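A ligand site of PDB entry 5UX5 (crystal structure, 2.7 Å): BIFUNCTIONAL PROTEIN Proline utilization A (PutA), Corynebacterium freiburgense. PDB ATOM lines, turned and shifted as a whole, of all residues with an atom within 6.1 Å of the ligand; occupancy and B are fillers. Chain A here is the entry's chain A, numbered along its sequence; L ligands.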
ATOM      1  N   ALA A 591      28.508  -8.933   6.883  1.00  0.00           N
ATOM      2  CA  ALA A 591      28.652  -7.519   6.564  1.00  0.00           C
ATOM      3  C   ALA A 591      27.257  -6.957   6.300  1.00  0.00           C
ATOM      4  O   ALA A 591      26.624  -7.315   5.308  1.00  0.00           O
ATOM      5  CB  ALA A 591      29.597  -7.320   5.384  1.00  0.00           C
ATOM      6  N   SER A 592      26.770  -6.130   7.207  1.00  0.00           N
ATOM      7  CA  SER A 592      25.372  -5.729   7.261  1.00  0.00           C
ATOM      8  C   SER A 592      25.195  -4.265   6.846  1.00  0.00           C
ATOM      9  O   SER A 592      26.159  -3.479   6.830  1.00  0.00           O
ATOM     10  CB  SER A 592      24.846  -5.933   8.690  1.00  0.00           C
ATOM     11  OG  SER A 592      25.587  -5.149   9.614  1.00  0.00           O
ATOM     12  N   PRO A 593      23.979  -3.871   6.441  1.00  0.00           N
ATOM     13  CA  PRO A 593      23.754  -2.481   6.005  1.00  0.00           C
ATOM     14  C   PRO A 593      23.223  -1.618   7.130  1.00  0.00           C
ATOM     15  O   PRO A 593      23.201  -2.073   8.289  1.00  0.00           O
ATOM     16  CB  PRO A 593      22.719  -2.637   4.892  1.00  0.00           C
ATOM     17  CG  PRO A 593      21.885  -3.831   5.387  1.00  0.00           C
ATOM     18  CD  PRO A 593      22.796  -4.714   6.206  1.00  0.00           C
ATOM     19  N   TRP A 594      22.762  -0.395   6.810  1.00  0.00           N
ATOM     20  CA  TRP A 594      22.251   0.544   7.806  1.00  0.00           C
ATOM     21  C   TRP A 594      20.727   0.647   7.841  1.00  0.00           C
ATOM     22  O   TRP A 594      20.184   0.978   8.887  1.00  0.00           O
ATOM     23  CB  TRP A 594      22.828   1.953   7.592  1.00  0.00           C
ATOM     24  CG  TRP A 594      22.734   2.400   6.187  1.00  0.00           C
ATOM     25  CD1 TRP A 594      23.724   2.403   5.288  1.00  0.00           C
ATOM     26  CD2 TRP A 594      21.566   2.895   5.519  1.00  0.00           C
ATOM     27  NE1 TRP A 594      23.269   2.867   4.079  1.00  0.00           N
ATOM     28  CE2 TRP A 594      21.944   3.170   4.185  1.00  0.00           C
ATOM     29  CE3 TRP A 594      20.251   3.143   5.907  1.00  0.00           C
ATOM     30  CZ2 TRP A 594      21.054   3.654   3.240  1.00  0.00           C
ATOM     31  CZ3 TRP A 594      19.356   3.619   4.959  1.00  0.00           C
ATOM     32  CH2 TRP A 594      19.777   3.878   3.635  1.00  0.00           C
ATOM     33  N   LYS A 618      30.367  -7.509  11.121  1.00  0.00           N
ATOM     34  CA  LYS A 618      30.962  -6.226  10.737  1.00  0.00           C
ATOM     35  C   LYS A 618      29.834  -5.295  10.293  1.00  0.00           C
ATOM     36  O   LYS A 618      29.405  -5.346   9.125  1.00  0.00           O
ATOM     37  CB  LYS A 618      32.018  -6.440   9.647  1.00  0.00           C
ATOM     38  CG  LYS A 618      32.902  -5.228   9.372  1.00  0.00           C
ATOM     39  CD  LYS A 618      32.306  -4.459   8.236  1.00  0.00           C
ATOM     40  CE  LYS A 618      32.524  -3.022   8.374  1.00  0.00           C
ATOM     41  NZ  LYS A 618      31.448  -2.415   7.567  1.00  0.00           N
ATOM     42  N   PRO A 619      29.337  -4.418  11.150  1.00  0.00           N
ATOM     43  CA  PRO A 619      28.157  -3.629  10.802  1.00  0.00           C
ATOM     44  C   PRO A 619      28.472  -2.390   9.974  1.00  0.00           C
ATOM     45  O   PRO A 619      29.585  -1.834   9.990  1.00  0.00           O
ATOM     46  CB  PRO A 619      27.595  -3.230  12.164  1.00  0.00           C
ATOM     47  CG  PRO A 619      28.751  -3.322  13.118  1.00  0.00           C
ATOM     48  CD  PRO A 619      29.887  -4.042  12.461  1.00  0.00           C
ATOM     49  N   ALA A 620      27.443  -1.920   9.266  1.00  0.00           N
ATOM     50  CA  ALA A 620      27.614  -0.742   8.429  1.00  0.00           C
ATOM     51  C   ALA A 620      28.016   0.449   9.299  1.00  0.00           C
ATOM     52  O   ALA A 620      27.470   0.642  10.390  1.00  0.00           O
ATOM     53  CB  ALA A 620      26.345  -0.426   7.652  1.00  0.00           C
ATOM     54  N   PRO A 621      28.951   1.273   8.857  1.00  0.00           N
ATOM     55  CA  PRO A 621      29.492   2.317   9.746  1.00  0.00           C
ATOM     56  C   PRO A 621      28.466   3.347  10.229  1.00  0.00           C
ATOM     57  O   PRO A 621      28.672   3.932  11.286  1.00  0.00           O
ATOM     58  CB  PRO A 621      30.592   2.966   8.895  1.00  0.00           C
ATOM     59  CG  PRO A 621      30.242   2.652   7.510  1.00  0.00           C
ATOM     60  CD  PRO A 621      29.568   1.316   7.525  1.00  0.00           C
ATOM     61  N   GLU A 622      27.354   3.548   9.521  1.00  0.00           N
ATOM     62  CA  GLU A 622      26.335   4.483   9.990  1.00  0.00           C
ATOM     63  C   GLU A 622      25.626   3.991  11.238  1.00  0.00           C
ATOM     64  O   GLU A 622      24.967   4.798  11.916  1.00  0.00           O
ATOM     65  CB  GLU A 622      25.282   4.739   8.902  1.00  0.00           C
ATOM     66  CG  GLU A 622      25.733   5.479   7.637  1.00  0.00           C
ATOM     67  CD  GLU A 622      26.478   4.575   6.648  1.00  0.00           C
ATOM     68  OE1 GLU A 622      26.597   3.367   6.897  1.00  0.00           O
ATOM     69  OE2 GLU A 622      26.936   5.083   5.595  1.00  0.00           O
ATOM     70  N   THR A 649      35.725  -2.905  11.642  1.00  0.00           N
ATOM     71  CA  THR A 649      36.828  -2.638  10.740  1.00  0.00           C
ATOM     72  C   THR A 649      36.481  -1.440   9.856  1.00  0.00           C
ATOM     73  O   THR A 649      35.311  -1.149   9.586  1.00  0.00           O
ATOM     74  CB  THR A 649      37.146  -3.839   9.823  1.00  0.00           C
ATOM     75  OG1 THR A 649      36.125  -3.976   8.825  1.00  0.00           O
ATOM     76  CG2 THR A 649      37.236  -5.138  10.622  1.00  0.00           C
ATOM     77  N   ASP A 650      37.530  -0.745   9.425  1.00  0.00           N
ATOM     78  CA  ASP A 650      37.368   0.275   8.419  1.00  0.00           C
ATOM     79  C   ASP A 650      37.048  -0.389   7.080  1.00  0.00           C
ATOM     80  O   ASP A 650      36.840  -1.600   7.001  1.00  0.00           O
ATOM     81  CB  ASP A 650      38.618   1.143   8.307  1.00  0.00           C
ATOM     82  CG  ASP A 650      39.863   0.336   8.026  1.00  0.00           C
ATOM     83  OD1 ASP A 650      39.732  -0.792   7.501  1.00  0.00           O
ATOM     84  OD2 ASP A 650      40.981   0.828   8.321  1.00  0.00           O
ATOM     85  N   GLU A 651      36.973   0.412   6.042  1.00  0.00           N
ATOM     86  CA  GLU A 651      36.853  -0.024   4.671  1.00  0.00           C
ATOM     87  C   GLU A 651      38.159   0.195   3.911  1.00  0.00           C
ATOM     88  O   GLU A 651      38.141   0.459   2.708  1.00  0.00           O
ATOM     89  CB  GLU A 651      35.687   0.688   4.004  1.00  0.00           C
ATOM     90  CG  GLU A 651      34.359   0.358   4.676  1.00  0.00           C
ATOM     91  CD  GLU A 651      33.164   0.950   3.954  1.00  0.00           C
ATOM     92  OE1 GLU A 651      32.015   0.764   4.439  1.00  0.00           O
ATOM     93  OE2 GLU A 651      33.342   1.566   2.874  1.00  0.00           O
ATOM     94  N   ALA A 652      39.266   0.175   4.628  1.00  0.00           N
ATOM     95  CA  ALA A 652      40.608   0.210   4.038  1.00  0.00           C
ATOM     96  C   ALA A 652      41.285  -1.134   4.297  1.00  0.00           C
ATOM     97  O   ALA A 652      40.596  -2.160   4.190  1.00  0.00           O
ATOM     98  CB  ALA A 652      41.359   1.420   4.545  1.00  0.00           C
ATOM     99  N   ALA A 654      42.230  -3.065   6.871  1.00  0.00           N
ATOM    100  CA  ALA A 654      41.669  -4.024   7.830  1.00  0.00           C
ATOM    101  C   ALA A 654      40.345  -4.611   7.361  1.00  0.00           C
ATOM    102  O   ALA A 654      40.102  -5.818   7.510  1.00  0.00           O
ATOM    103  CB  ALA A 654      41.504  -3.349   9.187  1.00  0.00           C
ATOM    104  N   GLY A 655      39.478  -3.803   6.763  1.00  0.00           N
ATOM    105  CA  GLY A 655      38.239  -4.353   6.232  1.00  0.00           C
ATOM    106  C   GLY A 655      38.504  -5.315   5.090  1.00  0.00           C
ATOM    107  O   GLY A 655      37.937  -6.410   5.047  1.00  0.00           O
ATOM    108  N   ARG A 656      39.379  -4.933   4.164  1.00  0.00           N
ATOM    109  CA  ARG A 656      39.701  -5.805   3.050  1.00  0.00           C
ATOM    110  C   ARG A 656      40.354  -7.093   3.542  1.00  0.00           C
ATOM    111  O   ARG A 656      40.054  -8.190   3.059  1.00  0.00           O
ATOM    112  CB  ARG A 656      40.628  -5.072   2.079  1.00  0.00           C
ATOM    113  CG  ARG A 656      41.259  -5.986   1.063  1.00  0.00           C
ATOM    114  CD  ARG A 656      41.812  -5.244  -0.133  1.00  0.00           C
ATOM    115  NE  ARG A 656      42.209  -6.183  -1.183  1.00  0.00           N
ATOM    116  CZ  ARG A 656      42.776  -5.813  -2.319  1.00  0.00           C
ATOM    117  NH1 ARG A 656      43.020  -4.533  -2.562  1.00  0.00           N
ATOM    118  NH2 ARG A 656      43.076  -6.727  -3.230  1.00  0.00           N
ATOM    119  N   MET A 659      37.474  -9.254   4.799  1.00  0.00           N
ATOM    120  CA  MET A 659      36.613  -9.878   3.792  1.00  0.00           C
ATOM    121  C   MET A 659      37.367 -10.856   2.919  1.00  0.00           C
ATOM    122  O   MET A 659      36.752 -11.771   2.361  1.00  0.00           O
ATOM    123  CB  MET A 659      35.937  -8.842   2.897  1.00  0.00           C
ATOM    124  CG  MET A 659      35.096  -7.859   3.636  1.00  0.00           C
ATOM    125  SD  MET A 659      33.954  -8.586   4.805  1.00  0.00           S
ATOM    126  CE  MET A 659      33.299  -7.087   5.572  1.00  0.00           C
ATOM    127  N   LEU A 669      26.333 -10.873   2.989  1.00  0.00           N
ATOM    128  CA  LEU A 669      26.418  -9.456   2.686  1.00  0.00           C
ATOM    129  C   LEU A 669      25.066  -8.927   2.228  1.00  0.00           C
ATOM    130  O   LEU A 669      24.371  -9.576   1.448  1.00  0.00           O
ATOM    131  CB  LEU A 669      27.435  -9.202   1.574  1.00  0.00           C
ATOM    132  CG  LEU A 669      27.430  -7.864   0.829  1.00  0.00           C
ATOM    133  CD1 LEU A 669      27.878  -6.782   1.755  1.00  0.00           C
ATOM    134  CD2 LEU A 669      28.344  -7.952  -0.410  1.00  0.00           C
ATOM    135  N   THR A 670      24.725  -7.733   2.701  1.00  0.00           N
ATOM    136  CA  THR A 670      23.528  -7.009   2.266  1.00  0.00           C
ATOM    137  C   THR A 670      23.971  -5.599   1.931  1.00  0.00           C
ATOM    138  O   THR A 670      24.381  -4.858   2.822  1.00  0.00           O
ATOM    139  CB  THR A 670      22.455  -6.973   3.340  1.00  0.00           C
ATOM    140  OG1 THR A 670      22.187  -8.306   3.812  1.00  0.00           O
ATOM    141  CG2 THR A 670      21.181  -6.333   2.796  1.00  0.00           C
ATOM    142  N   GLY A 671      23.879  -5.222   0.673  1.00  0.00           N
ATOM    143  CA  GLY A 671      24.374  -3.919   0.259  1.00  0.00           C
ATOM    144  C   GLY A 671      24.347  -3.775  -1.242  1.00  0.00           C
ATOM    145  O   GLY A 671      23.457  -4.307  -1.916  1.00  0.00           O
ATOM    146  N   ALA A 672      25.312  -3.073  -1.754  1.00  0.00           N
ATOM    147  CA  ALA A 672      25.327  -2.790  -3.176  1.00  0.00           C
ATOM    148  C   ALA A 672      25.919  -3.959  -3.951  1.00  0.00           C
ATOM    149  O   ALA A 672      26.889  -4.587  -3.525  1.00  0.00           O
ATOM    150  CB  ALA A 672      26.128  -1.527  -3.431  1.00  0.00           C
ATOM    151  N   SER A 673      25.346  -4.257  -5.117  1.00  0.00           N
ATOM    152  CA  SER A 673      25.937  -5.302  -5.926  1.00  0.00           C
ATOM    153  C   SER A 673      27.354  -4.947  -6.360  1.00  0.00           C
ATOM    154  O   SER A 673      28.155  -5.853  -6.620  1.00  0.00           O
ATOM    155  CB  SER A 673      25.033  -5.595  -7.129  1.00  0.00           C
ATOM    156  OG  SER A 673      24.762  -4.420  -7.848  1.00  0.00           O
ATOM    157  N   THR A 675      29.493  -3.695  -4.306  1.00  0.00           N
ATOM    158  CA  THR A 675      30.261  -4.163  -3.166  1.00  0.00           C
ATOM    159  C   THR A 675      30.496  -5.666  -3.229  1.00  0.00           C
ATOM    160  O   THR A 675      31.593  -6.144  -2.903  1.00  0.00           O
ATOM    161  CB  THR A 675      29.521  -3.748  -1.897  1.00  0.00           C
ATOM    162  OG1 THR A 675      29.487  -2.313  -1.860  1.00  0.00           O
ATOM    163  CG2 THR A 675      30.198  -4.271  -0.672  1.00  0.00           C
ATOM    164  N   ALA A 676      29.488  -6.424  -3.650  1.00  0.00           N
ATOM    165  CA  ALA A 676      29.673  -7.866  -3.796  1.00  0.00           C
ATOM    166  C   ALA A 676      30.738  -8.179  -4.834  1.00  0.00           C
ATOM    167  O   ALA A 676      31.585  -9.052  -4.595  1.00  0.00           O
ATOM    168  CB  ALA A 676      28.353  -8.546  -4.127  1.00  0.00           C
ATOM    169  N   LEU A 678      33.171  -6.218  -5.653  1.00  0.00           N
ATOM    170  CA  LEU A 678      34.425  -5.777  -5.051  1.00  0.00           C
ATOM    171  C   LEU A 678      35.028  -6.869  -4.185  1.00  0.00           C
ATOM    172  O   LEU A 678      36.176  -7.296  -4.402  1.00  0.00           O
ATOM    173  CB  LEU A 678      34.170  -4.526  -4.228  1.00  0.00           C
ATOM    174  CG  LEU A 678      35.387  -3.912  -3.552  1.00  0.00           C
ATOM    175  CD1 LEU A 678      36.216  -3.168  -4.564  1.00  0.00           C
ATOM    176  CD2 LEU A 678      34.909  -2.996  -2.451  1.00  0.00           C
ATOM    177  N   PHE A 679      34.266  -7.342  -3.188  1.00  0.00           N
ATOM    178  CA  PHE A 679      34.754  -8.375  -2.277  1.00  0.00           C
ATOM    179  C   PHE A 679      35.236  -9.592  -3.048  1.00  0.00           C
ATOM    180  O   PHE A 679      36.352 -10.091  -2.822  1.00  0.00           O
ATOM    181  CB  PHE A 679      33.649  -8.795  -1.291  1.00  0.00           C
ATOM    182  CG  PHE A 679      33.249  -7.732  -0.277  1.00  0.00           C
ATOM    183  CD1 PHE A 679      33.876  -6.500  -0.233  1.00  0.00           C
ATOM    184  CD2 PHE A 679      32.239  -8.000   0.648  1.00  0.00           C
ATOM    185  CE1 PHE A 679      33.504  -5.543   0.732  1.00  0.00           C
ATOM    186  CE2 PHE A 679      31.864  -7.059   1.599  1.00  0.00           C
ATOM    187  CZ  PHE A 679      32.494  -5.819   1.646  1.00  0.00           C
ATOM    188  N   TRP A 682      38.596  -9.743  -4.698  1.00  0.00           N
ATOM    189  CA  TRP A 682      39.728  -9.991  -3.804  1.00  0.00           C
ATOM    190  C   TRP A 682      39.966 -11.470  -3.531  1.00  0.00           C
ATOM    191  O   TRP A 682      41.051 -11.823  -3.043  1.00  0.00           O
ATOM    192  CB  TRP A 682      39.535  -9.320  -2.457  1.00  0.00           C
ATOM    193  CG  TRP A 682      39.381  -7.864  -2.517  1.00  0.00           C
ATOM    194  CD1 TRP A 682      39.884  -7.060  -3.462  1.00  0.00           C
ATOM    195  CD2 TRP A 682      38.683  -7.036  -1.589  1.00  0.00           C
ATOM    196  NE1 TRP A 682      39.558  -5.758  -3.189  1.00  0.00           N
ATOM    197  CE2 TRP A 682      38.812  -5.716  -2.044  1.00  0.00           C
ATOM    198  CE3 TRP A 682      37.954  -7.282  -0.412  1.00  0.00           C
ATOM    199  CZ2 TRP A 682      38.241  -4.626  -1.376  1.00  0.00           C
ATOM    200  CZ3 TRP A 682      37.380  -6.214   0.255  1.00  0.00           C
ATOM    201  CH2 TRP A 682      37.523  -4.899  -0.240  1.00  0.00           C
ATOM    202  N   SER A 693      19.576  -5.253  -3.119  1.00  0.00           N
ATOM    203  CA  SER A 693      18.629  -4.208  -3.526  1.00  0.00           C
ATOM    204  C   SER A 693      17.730  -4.657  -4.676  1.00  0.00           C
ATOM    205  O   SER A 693      17.934  -5.728  -5.269  1.00  0.00           O
ATOM    206  CB  SER A 693      19.387  -2.925  -3.895  1.00  0.00           C
ATOM    207  OG  SER A 693      18.521  -1.859  -4.225  1.00  0.00           O
ATOM    208  N   GLU A 819      17.692   1.934  -8.985  1.00  0.00           N
ATOM    209  CA  GLU A 819      17.126   2.041  -7.647  1.00  0.00           C
ATOM    210  C   GLU A 819      17.778   3.220  -6.948  1.00  0.00           C
ATOM    211  O   GLU A 819      19.000   3.251  -6.772  1.00  0.00           O
ATOM    212  CB  GLU A 819      17.337   0.758  -6.842  1.00  0.00           C
ATOM    213  CG  GLU A 819      18.679   0.018  -7.036  1.00  0.00           C
ATOM    214  CD  GLU A 819      19.756   0.395  -6.019  1.00  0.00           C
ATOM    215  OE1 GLU A 819      19.414   0.597  -4.840  1.00  0.00           O
ATOM    216  OE2 GLU A 819      20.954   0.480  -6.407  1.00  0.00           O
ATOM    217  N   CYS A 820      16.959   4.232  -6.593  1.00  0.00           N
ATOM    218  CA  CYS A 820      17.446   5.414  -5.886  1.00  0.00           C
ATOM    219  C   CYS A 820      17.472   5.279  -4.375  1.00  0.00           C
ATOM    220  O   CYS A 820      18.195   6.034  -3.720  1.00  0.00           O
ATOM    221  CB  CYS A 820      16.622   6.630  -6.256  1.00  0.00           C
ATOM    222  SG  CYS A 820      16.783   7.025  -7.953  1.00  0.00           S
ATOM    223  N   PHE A 821      16.743   4.334  -3.797  1.00  0.00           N
ATOM    224  CA  PHE A 821      16.806   4.120  -2.355  1.00  0.00           C
ATOM    225  C   PHE A 821      16.412   5.384  -1.581  1.00  0.00           C
ATOM    226  O   PHE A 821      17.091   5.815  -0.658  1.00  0.00           O
ATOM    227  CB  PHE A 821      18.196   3.633  -1.933  1.00  0.00           C
ATOM    228  CG  PHE A 821      18.183   2.422  -1.055  1.00  0.00           C
ATOM    229  CD1 PHE A 821      17.839   1.184  -1.579  1.00  0.00           C
ATOM    230  CD2 PHE A 821      18.516   2.519   0.290  1.00  0.00           C
ATOM    231  CE1 PHE A 821      17.811   0.037  -0.782  1.00  0.00           C
ATOM    232  CE2 PHE A 821      18.500   1.366   1.084  1.00  0.00           C
ATOM    233  CZ  PHE A 821      18.139   0.131   0.546  1.00  0.00           C
HETATM  234  P1  LIG L   1      27.746  -1.209   0.912  1.00  0.00           P
HETATM  235  O1  LIG L   1      27.264  -2.234  -0.174  1.00  0.00           O
HETATM  236  O2  LIG L   1      28.869  -0.300   0.323  1.00  0.00           O
HETATM  237  O3  LIG L   1      28.359  -1.977   2.140  1.00  0.00           O
HETATM  238  C1  LIG L   1      27.601  -2.761   3.031  1.00  0.00           C
HETATM  239  C2  LIG L   1      28.515  -3.384   4.081  1.00  0.00           C
HETATM  240  O4  LIG L   1      29.768  -3.839   3.565  1.00  0.00           O
HETATM  241  C3  LIG L   1      28.776  -2.436   5.212  1.00  0.00           C
HETATM  242  O5  LIG L   1      28.960  -3.106   6.408  1.00  0.00           O
HETATM  243  C4  LIG L   1      30.008  -1.820   4.690  1.00  0.00           C
HETATM  244  O6  LIG L   1      30.704  -1.037   5.590  1.00  0.00           O
HETATM  245  C5  LIG L   1      30.748  -3.023   4.191  1.00  0.00           C
HETATM  246  N1  LIG L   1      31.830  -2.680   3.281  1.00  0.00           N
HETATM  247  C6  LIG L   1      31.729  -2.055   2.052  1.00  0.00           C
HETATM  248  N2  LIG L   1      32.949  -1.898   1.511  1.00  0.00           N
HETATM  249  C7  LIG L   1      33.926  -2.435   2.374  1.00  0.00           C
HETATM  250  C8  LIG L   1      35.309  -2.578   2.331  1.00  0.00           C
HETATM  251  N3  LIG L   1      36.109  -2.088   1.234  1.00  0.00           N
HETATM  252  N4  LIG L   1      35.934  -3.166   3.363  1.00  0.00           N
HETATM  253  C9  LIG L   1      35.261  -3.636   4.445  1.00  0.00           C
HETATM  254  N5  LIG L   1      33.904  -3.530   4.512  1.00  0.00           N
HETATM  255  C10 LIG L   1      33.220  -2.945   3.509  1.00  0.00           C
HETATM  256  O7  LIG L   1      26.425  -0.437   1.392  1.00  0.00           O
HETATM  257  P2  LIG L   1      26.247   1.118   1.795  1.00  0.00           P
HETATM  258  O8  LIG L   1      27.465   1.976   1.542  1.00  0.00           O
HETATM  259  O9  LIG L   1      26.082   1.173   3.281  1.00  0.00           O
HETATM  260  O10 LIG L   1      24.964   1.619   0.969  1.00  0.00           O
HETATM  261  C11 LIG L   1      25.023   1.549  -0.448  1.00  0.00           C
HETATM  262  C12 LIG L   1      23.708   1.281  -1.187  1.00  0.00           C
HETATM  263  O11 LIG L   1      23.094   0.051  -0.911  1.00  0.00           O
HETATM  264  C13 LIG L   1      22.599   2.256  -0.999  1.00  0.00           C
HETATM  265  O12 LIG L   1      22.845   3.529  -1.473  1.00  0.00           O
HETATM  266  C14 LIG L   1      21.603   1.575  -1.853  1.00  0.00           C
HETATM  267  O13 LIG L   1      21.662   2.104  -3.127  1.00  0.00           O
HETATM  268  C15 LIG L   1      21.959   0.112  -1.757  1.00  0.00           C
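O of Lys 618 lies within hydrogen-bond range of N of Ser 592 (3.4 Å).
The backbone NH of Ala 620 sits at hydrogen-bond distance from the backbone carbonyl oxygen of Ser 592 (3.2 Å).
The side-chain hydroxyl (OG) of Ser 693 sits at hydrogen-bond distance from the side-chain carboxylate (OE1) of Glu 819.
The backbone NH (N) of Gly 655 is in hydrogen-bond range of the side-chain carboxylate (OD1) of Asp 650, 3.1 Å away.
N of Ala 652 lies within hydrogen-bond range of OD1 of Asp 650 (3.1 Å).
The side-chain carboxylate (OD1) of Asp 650 is in hydrogen-bond range of the backbone NH (N) of Ala 654 (3.4 Å).
The backbone NH (N) of Thr 670 lies within hydrogen-bond range of the backbone carbonyl oxygen (O) of Ala 591 (3.3 Å).
An oxygen (O6) of the ligand lies within hydrogen-bond range of the side-chain carboxylate (OE1) of Glu 651 (2.5 Å).
The side-chain amino group (NZ) of Lys 618 is in hydrogen-bond range of an oxygen (O6) of the ligand (2.5 Å).
N of Ala 672 is in hydrogen-bond range of O1 of the ligand (2.6 Å).
The side-chain hydroxyl of Thr 675 sits at hydrogen-bond distance from an oxygen (O1) of the ligand (2.8 Å).
An oxygen (O5) of the ligand is in hydrogen-bond range of the backbone carbonyl oxygen (O) of Ser 592 (2.9 Å).
The side-chain carboxylate of Glu 819 sits at hydrogen-bond distance from an oxygen (O13) of the ligand, at 3.2 Å.
The indole nitrogen (NE1) of Trp 594 sits close to an oxygen (O9) of the ligand, 3.4 Å away.
The backbone NH (N) of Ala 620 lies close to an oxygen (O5) of the ligand.
Residues that only touch the ligand: Pro 621, Gly 671, Trp 682, Phe 679, Gly 655, Phe 821, Asp 650, Pro 619, Met 659, Thr 670, Ala 591, Leu 669, Arg 656 and Leu 678.
Of the 31 residues printed, 22 come within 4 Å of the ligand.
The nearest printed residue that does not touch the ligand is Glu 622 (4.3 Å).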
